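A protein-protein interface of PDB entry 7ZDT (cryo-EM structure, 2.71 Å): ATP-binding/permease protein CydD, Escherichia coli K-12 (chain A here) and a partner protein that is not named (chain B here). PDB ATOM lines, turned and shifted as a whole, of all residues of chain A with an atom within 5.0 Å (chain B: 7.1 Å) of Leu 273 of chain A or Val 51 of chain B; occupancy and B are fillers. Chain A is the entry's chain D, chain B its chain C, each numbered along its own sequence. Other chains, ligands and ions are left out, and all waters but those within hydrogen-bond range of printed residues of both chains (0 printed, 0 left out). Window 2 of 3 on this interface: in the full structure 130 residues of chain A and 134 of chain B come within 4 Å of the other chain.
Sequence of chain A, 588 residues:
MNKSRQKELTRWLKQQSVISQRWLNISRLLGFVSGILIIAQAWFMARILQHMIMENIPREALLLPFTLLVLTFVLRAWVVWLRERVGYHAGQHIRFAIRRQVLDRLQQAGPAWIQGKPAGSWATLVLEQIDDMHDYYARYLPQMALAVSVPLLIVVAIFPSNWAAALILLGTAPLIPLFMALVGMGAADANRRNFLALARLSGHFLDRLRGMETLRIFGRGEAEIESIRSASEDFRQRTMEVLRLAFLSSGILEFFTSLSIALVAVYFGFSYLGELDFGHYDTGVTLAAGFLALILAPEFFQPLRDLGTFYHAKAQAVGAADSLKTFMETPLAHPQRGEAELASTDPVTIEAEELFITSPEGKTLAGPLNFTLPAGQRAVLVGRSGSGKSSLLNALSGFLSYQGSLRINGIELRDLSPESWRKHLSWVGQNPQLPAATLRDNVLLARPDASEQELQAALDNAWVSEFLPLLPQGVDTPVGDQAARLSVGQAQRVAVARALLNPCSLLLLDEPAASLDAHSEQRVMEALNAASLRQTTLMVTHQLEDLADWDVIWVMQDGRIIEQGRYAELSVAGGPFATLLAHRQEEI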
ATOM      1  N   GLY A 269      24.444  16.130  31.001  1.00  0.00           N
ATOM      2  CA  GLY A 269      24.291  16.748  29.696  1.00  0.00           C
ATOM      3  C   GLY A 269      23.334  17.923  29.714  1.00  0.00           C
ATOM      4  O   GLY A 269      23.599  18.961  29.106  1.00  0.00           O
ATOM      5  N   PHE A 270      22.209  17.778  30.414  1.00  0.00           N
ATOM      6  CA  PHE A 270      21.266  18.885  30.520  1.00  0.00           C
ATOM      7  C   PHE A 270      21.773  19.958  31.472  1.00  0.00           C
ATOM      8  O   PHE A 270      21.468  21.140  31.291  1.00  0.00           O
ATOM      9  CB  PHE A 270      19.898  18.375  30.974  1.00  0.00           C
ATOM     10  CG  PHE A 270      19.182  17.545  29.945  1.00  0.00           C
ATOM     11  CD1 PHE A 270      17.968  16.953  30.241  1.00  0.00           C
ATOM     12  CD2 PHE A 270      19.717  17.357  28.683  1.00  0.00           C
ATOM     13  CE1 PHE A 270      17.306  16.189  29.301  1.00  0.00           C
ATOM     14  CE2 PHE A 270      19.060  16.593  27.742  1.00  0.00           C
ATOM     15  CZ  PHE A 270      17.854  16.009  28.052  1.00  0.00           C
ATOM     16  N   SER A 271      22.536  19.566  32.493  1.00  0.00           N
ATOM     17  CA  SER A 271      23.096  20.540  33.424  1.00  0.00           C
ATOM     18  C   SER A 271      24.104  21.450  32.737  1.00  0.00           C
ATOM     19  O   SER A 271      24.147  22.655  33.011  1.00  0.00           O
ATOM     20  CB  SER A 271      23.744  19.822  34.606  1.00  0.00           C
ATOM     21  OG  SER A 271      24.041  20.728  35.650  1.00  0.00           O
ATOM     22  N   TYR A 272      24.931  20.890  31.851  1.00  0.00           N
ATOM     23  CA  TYR A 272      25.917  21.702  31.144  1.00  0.00           C
ATOM     24  C   TYR A 272      25.242  22.743  30.265  1.00  0.00           C
ATOM     25  O   TYR A 272      25.677  23.899  30.209  1.00  0.00           O
ATOM     26  CB  TYR A 272      26.829  20.809  30.303  1.00  0.00           C
ATOM     27  CG  TYR A 272      27.787  19.969  31.112  1.00  0.00           C
ATOM     28  CD1 TYR A 272      28.510  20.521  32.155  1.00  0.00           C
ATOM     29  CD2 TYR A 272      27.977  18.629  30.821  1.00  0.00           C
ATOM     30  CE1 TYR A 272      29.384  19.758  32.892  1.00  0.00           C
ATOM     31  CE2 TYR A 272      28.847  17.859  31.554  1.00  0.00           C
ATOM     32  CZ  TYR A 272      29.549  18.428  32.586  1.00  0.00           C
ATOM     33  OH  TYR A 272      30.421  17.663  33.319  1.00  0.00           O
ATOM     34  N   LEU A 273      24.177  22.349  29.565  1.00  0.00           N
ATOM     35  CA  LEU A 273      23.485  23.275  28.677  1.00  0.00           C
ATOM     36  C   LEU A 273      22.727  24.342  29.454  1.00  0.00           C
ATOM     37  O   LEU A 273      22.417  25.404  28.905  1.00  0.00           O
ATOM     38  CB  LEU A 273      22.525  22.508  27.771  1.00  0.00           C
ATOM     39  CG  LEU A 273      23.162  21.498  26.822  1.00  0.00           C
ATOM     40  CD1 LEU A 273      22.098  20.842  25.982  1.00  0.00           C
ATOM     41  CD2 LEU A 273      24.194  22.177  25.944  1.00  0.00           C
ATOM     42  N   GLY A 274      22.423  24.085  30.719  1.00  0.00           N
ATOM     43  CA  GLY A 274      21.617  24.987  31.506  1.00  0.00           C
ATOM     44  C   GLY A 274      20.155  24.622  31.604  1.00  0.00           C
ATOM     45  O   GLY A 274      19.367  25.439  32.090  1.00  0.00           O
ATOM     46  N   GLU A 275      19.767  23.430  31.147  1.00  0.00           N
ATOM     47  CA  GLU A 275      18.369  23.018  31.227  1.00  0.00           C
ATOM     48  C   GLU A 275      17.920  22.888  32.677  1.00  0.00           C
ATOM     49  O   GLU A 275      16.786  23.233  33.023  1.00  0.00           O
ATOM     50  CB  GLU A 275      18.172  21.701  30.479  1.00  0.00           C
ATOM     51  CG  GLU A 275      18.333  21.817  28.975  1.00  0.00           C
ATOM     52  CD  GLU A 275      17.233  22.631  28.334  1.00  0.00           C
ATOM     53  OE1 GLU A 275      16.094  22.596  28.844  1.00  0.00           O
ATOM     54  OE2 GLU A 275      17.505  23.302  27.319  1.00  0.00           O
ATOM     55  N   PHE B  42      28.364  12.848  24.516  1.00  0.00           N
ATOM     56  CA  PHE B  42      27.261  13.747  24.840  1.00  0.00           C
ATOM     57  C   PHE B  42      27.646  14.716  25.949  1.00  0.00           C
ATOM     58  O   PHE B  42      27.336  15.909  25.874  1.00  0.00           O
ATOM     59  CB  PHE B  42      26.027  12.936  25.232  1.00  0.00           C
ATOM     60  CG  PHE B  42      24.846  13.770  25.629  1.00  0.00           C
ATOM     61  CD1 PHE B  42      24.530  14.926  24.944  1.00  0.00           C
ATOM     62  CD2 PHE B  42      24.038  13.384  26.682  1.00  0.00           C
ATOM     63  CE1 PHE B  42      23.443  15.687  25.311  1.00  0.00           C
ATOM     64  CE2 PHE B  42      22.951  14.140  27.051  1.00  0.00           C
ATOM     65  CZ  PHE B  42      22.653  15.293  26.365  1.00  0.00           C
ATOM     66  N   ALA B  45      30.273  17.170  24.393  1.00  0.00           N
ATOM     67  CA  ALA B  45      29.640  18.079  23.443  1.00  0.00           C
ATOM     68  C   ALA B  45      28.759  19.098  24.151  1.00  0.00           C
ATOM     69  O   ALA B  45      28.751  20.278  23.788  1.00  0.00           O
ATOM     70  CB  ALA B  45      28.829  17.289  22.419  1.00  0.00           C
ATOM     71  N   SER B  46      28.002  18.659  25.158  1.00  0.00           N
ATOM     72  CA  SER B  46      27.171  19.585  25.919  1.00  0.00           C
ATOM     73  C   SER B  46      28.020  20.584  26.693  1.00  0.00           C
ATOM     74  O   SER B  46      27.688  21.773  26.756  1.00  0.00           O
ATOM     75  CB  SER B  46      26.259  18.812  26.867  1.00  0.00           C
ATOM     76  OG  SER B  46      25.195  18.205  26.161  1.00  0.00           O
ATOM     77  N   ALA B  47      29.115  20.118  27.299  1.00  0.00           N
ATOM     78  CA  ALA B  47      29.969  21.014  28.072  1.00  0.00           C
ATOM     79  C   ALA B  47      30.616  22.065  27.184  1.00  0.00           C
ATOM     80  O   ALA B  47      30.694  23.241  27.558  1.00  0.00           O
ATOM     81  CB  ALA B  47      31.034  20.211  28.814  1.00  0.00           C
ATOM     82  N   VAL B  48      31.094  21.662  26.006  1.00  0.00           N
ATOM     83  CA  VAL B  48      31.726  22.614  25.098  1.00  0.00           C
ATOM     84  C   VAL B  48      30.706  23.619  24.580  1.00  0.00           C
ATOM     85  O   VAL B  48      30.986  24.821  24.498  1.00  0.00           O
ATOM     86  CB  VAL B  48      32.421  21.866  23.946  1.00  0.00           C
ATOM     87  CG1 VAL B  48      32.819  22.830  22.849  1.00  0.00           C
ATOM     88  CG2 VAL B  48      33.636  21.129  24.463  1.00  0.00           C
ATOM     89  N   ALA B  49      29.507  23.146  24.225  1.00  0.00           N
ATOM     90  CA  ALA B  49      28.465  24.052  23.758  1.00  0.00           C
ATOM     91  C   ALA B  49      28.076  25.053  24.839  1.00  0.00           C
ATOM     92  O   ALA B  49      27.912  26.246  24.561  1.00  0.00           O
ATOM     93  CB  ALA B  49      27.246  23.256  23.299  1.00  0.00           C
ATOM     94  N   GLY B  50      27.928  24.587  26.075  1.00  0.00           N
ATOM     95  CA  GLY B  50      27.624  25.491  27.161  1.00  0.00           C
ATOM     96  C   GLY B  50      26.203  26.025  27.087  1.00  0.00           C
ATOM     97  O   GLY B  50      25.357  25.548  26.326  1.00  0.00           O
ATOM     98  N   VAL B  51      25.950  27.043  27.908  1.00  0.00           N
ATOM     99  CA  VAL B  51      24.631  27.668  27.940  1.00  0.00           C
ATOM    100  C   VAL B  51      24.362  28.422  26.644  1.00  0.00           C
ATOM    101  O   VAL B  51      23.234  28.431  26.136  1.00  0.00           O
ATOM    102  CB  VAL B  51      24.509  28.585  29.169  1.00  0.00           C
ATOM    103  CG1 VAL B  51      23.181  29.322  29.159  1.00  0.00           C
ATOM    104  CG2 VAL B  51      24.667  27.780  30.449  1.00  0.00           C
ATOM    105  N   ALA B  52      25.392  29.062  26.086  1.00  0.00           N
ATOM    106  CA  ALA B  52      25.215  29.864  24.879  1.00  0.00           C
ATOM    107  C   ALA B  52      24.744  29.013  23.705  1.00  0.00           C
ATOM    108  O   ALA B  52      23.881  29.430  22.925  1.00  0.00           O
ATOM    109  CB  ALA B  52      26.520  30.581  24.533  1.00  0.00           C
ATOM    110  N   GLY B  53      25.299  27.816  23.567  1.00  0.00           N
ATOM    111  CA  GLY B  53      24.967  26.922  22.481  1.00  0.00           C
ATOM    112  C   GLY B  53      23.779  26.021  22.727  1.00  0.00           C
ATOM    113  O   GLY B  53      23.640  25.007  22.035  1.00  0.00           O
ATOM    114  N   LEU B  54      22.925  26.352  23.696  1.00  0.00           N
ATOM    115  CA  LEU B  54      21.771  25.513  24.006  1.00  0.00           C
ATOM    116  C   LEU B  54      20.863  25.350  22.792  1.00  0.00           C
ATOM    117  O   LEU B  54      20.508  24.228  22.413  1.00  0.00           O
ATOM    118  CB  LEU B  54      20.998  26.114  25.182  1.00  0.00           C
ATOM    119  CG  LEU B  54      19.796  25.371  25.774  1.00  0.00           C
ATOM    120  CD1 LEU B  54      19.672  25.700  27.249  1.00  0.00           C
ATOM    121  CD2 LEU B  54      18.498  25.721  25.056  1.00  0.00           C
ATOM    122  N   TYR B  55      20.477  26.465  22.170  1.00  0.00           N
ATOM    123  CA  TYR B  55      19.490  26.410  21.095  1.00  0.00           C
ATOM    124  C   TYR B  55      20.077  25.796  19.829  1.00  0.00           C
ATOM    125  O   TYR B  55      19.349  25.195  19.032  1.00  0.00           O
ATOM    126  CB  TYR B  55      18.946  27.810  20.818  1.00  0.00           C
ATOM    127  CG  TYR B  55      18.104  28.363  21.947  1.00  0.00           C
ATOM    128  CD1 TYR B  55      18.696  28.984  23.039  1.00  0.00           C
ATOM    129  CD2 TYR B  55      16.720  28.258  21.925  1.00  0.00           C
ATOM    130  CE1 TYR B  55      17.935  29.486  24.074  1.00  0.00           C
ATOM    131  CE2 TYR B  55      15.950  28.758  22.957  1.00  0.00           C
ATOM    132  CZ  TYR B  55      16.563  29.371  24.029  1.00  0.00           C
ATOM    133  OH  TYR B  55      15.800  29.872  25.062  1.00  0.00           O
ATOM    134  N   PHE B  57      22.309  23.363  19.824  1.00  0.00           N
ATOM    135  CA  PHE B  57      22.708  21.987  20.089  1.00  0.00           C
ATOM    136  C   PHE B  57      21.479  21.090  20.149  1.00  0.00           C
ATOM    137  O   PHE B  57      20.540  21.360  20.904  1.00  0.00           O
ATOM    138  CB  PHE B  57      23.492  21.901  21.400  1.00  0.00           C
ATOM    139  CG  PHE B  57      24.021  20.531  21.704  1.00  0.00           C
ATOM    140  CD1 PHE B  57      24.982  19.950  20.897  1.00  0.00           C
ATOM    141  CD2 PHE B  57      23.555  19.825  22.797  1.00  0.00           C
ATOM    142  CE1 PHE B  57      25.467  18.689  21.175  1.00  0.00           C
ATOM    143  CE2 PHE B  57      24.038  18.565  23.078  1.00  0.00           C
ATOM    144  CZ  PHE B  57      24.995  17.997  22.268  1.00  0.00           C
ATOM    145  N   ASN B  58      21.491  20.021  19.350  1.00  0.00           N
ATOM    146  CA  ASN B  58      20.403  19.042  19.338  1.00  0.00           C
ATOM    147  C   ASN B  58      20.660  18.008  20.434  1.00  0.00           C
ATOM    148  O   ASN B  58      21.271  16.959  20.226  1.00  0.00           O
ATOM    149  CB  ASN B  58      20.286  18.388  17.968  1.00  0.00           C
ATOM    150  CG  ASN B  58      19.164  17.368  17.900  1.00  0.00           C
ATOM    151  OD1 ASN B  58      18.316  17.295  18.789  1.00  0.00           O
ATOM    152  ND2 ASN B  58      19.159  16.569  16.842  1.00  0.00           N
ATOM    153  N   TYR B  59      20.175  18.332  21.632  1.00  0.00           N
ATOM    154  CA  TYR B  59      20.405  17.471  22.786  1.00  0.00           C
ATOM    155  C   TYR B  59      19.347  16.389  22.945  1.00  0.00           C
ATOM    156  O   TYR B  59      19.555  15.450  23.717  1.00  0.00           O
ATOM    157  CB  TYR B  59      20.492  18.320  24.053  1.00  0.00           C
ATOM    158  CG  TYR B  59      19.231  19.090  24.386  1.00  0.00           C
ATOM    159  CD1 TYR B  59      18.183  18.492  25.071  1.00  0.00           C
ATOM    160  CD2 TYR B  59      19.093  20.419  24.012  1.00  0.00           C
ATOM    161  CE1 TYR B  59      17.036  19.197  25.376  1.00  0.00           C
ATOM    162  CE2 TYR B  59      17.950  21.130  24.310  1.00  0.00           C
ATOM    163  CZ  TYR B  59      16.924  20.515  24.992  1.00  0.00           C
ATOM    164  OH  TYR B  59      15.782  21.220  25.291  1.00  0.00           O
ATOM    165  N   MET B  60      18.217  16.498  22.243  1.00  0.00           N
ATOM    166  CA  MET B  60      17.166  15.497  22.392  1.00  0.00           C
ATOM    167  C   MET B  60      17.568  14.162  21.778  1.00  0.00           C
ATOM    168  O   MET B  60      17.269  13.103  22.340  1.00  0.00           O
ATOM    169  CB  MET B  60      15.863  16.001  21.777  1.00  0.00           C
ATOM    170  CG  MET B  60      15.268  17.198  22.491  1.00  0.00           C
ATOM    171  SD  MET B  60      14.863  16.825  24.209  1.00  0.00           S
ATOM    172  CE  MET B  60      13.487  15.697  24.002  1.00  0.00           C
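The side-chain hydroxyl (OG) of Ser 46 of chain B sits at hydrogen-bond distance from the backbone carbonyl oxygen (O) of Gly 269 of chain A, at 3.4 Å. The side-chain hydroxyl of Tyr 59 of chain B is in hydrogen-bond range of the side-chain carboxylate of Glu 275 of chain A, at 3.4 Å.
O of Phe 42 of chain B sits at hydrogen-bond distance from OG of Ser 46 of chain B (3.2 Å). The backbone carbonyl oxygen of Phe 270 of chain A lies within hydrogen-bond range of the backbone NH of Glu 275 of chain A.
CA of Gly 269 of chain A touches CE2 of Phe 42 of chain B, at 3.9 Å. CE2 of Phe 270 of chain A touches CD1 of Tyr 59 of chain B (3.4 Å). Tyr 272 of chain A touches Ser 46 of chain B. Tyr 272 of chain A touches Ala 47 of chain B. Gly 50 of chain B touches Tyr 272 of chain A (C to O, 3.8 Å). Tyr 272 of chain A touches Val 51 of chain B (O to N, 3.9 Å). Ser 46 of chain B touches Leu 273 of chain A. O of Leu 273 of chain A touches CD1 of Leu 54 of chain B, at 3.2 Å. Leu 273 of chain A touches Phe 57 of chain B (CD1 to CD2, 3.6 Å). Glu 275 of chain A touches Leu 54 of chain B (OE2 to CD1, 3.2 Å).
Printed residues of chain B within 4 Å of Phe 270 of chain A: Tyr 59. Printed residues of chain B within 4 Å of Tyr 272 of chain A: Ser 46, Ala 47, Gly 50 and Val 51. Of the printed residues of chain B, Leu 273 of chain A touches Ser 46 (3.6 Å), Gly 50 (3.6 Å), Val 51 (3.3 Å), Leu 54 (3.2 Å), Phe 57 (3.6 Å) and Tyr 59 (3.6 Å). Of the printed residues of chain A, Val 51 of chain B touches Tyr 272 and Leu 273. Printed residues of chain A within 4 Å of Leu 54 of chain B: Leu 273 (3.2 Å) and Glu 275 (3.2 Å).
Hydrophobic or aromatic side chains of chain B within 4 Å of the printed part of chain A: Phe 42, Ala 47, Val 51, Leu 54, Phe 57 and Tyr 59. Of the 7 printed residues of chain A, 5 touch a printed residue of chain B. Among the printed residues, no Asp or Glu carboxylate lies within 4 Å of a Lys or Arg side-chain nitrogen of the other chain.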
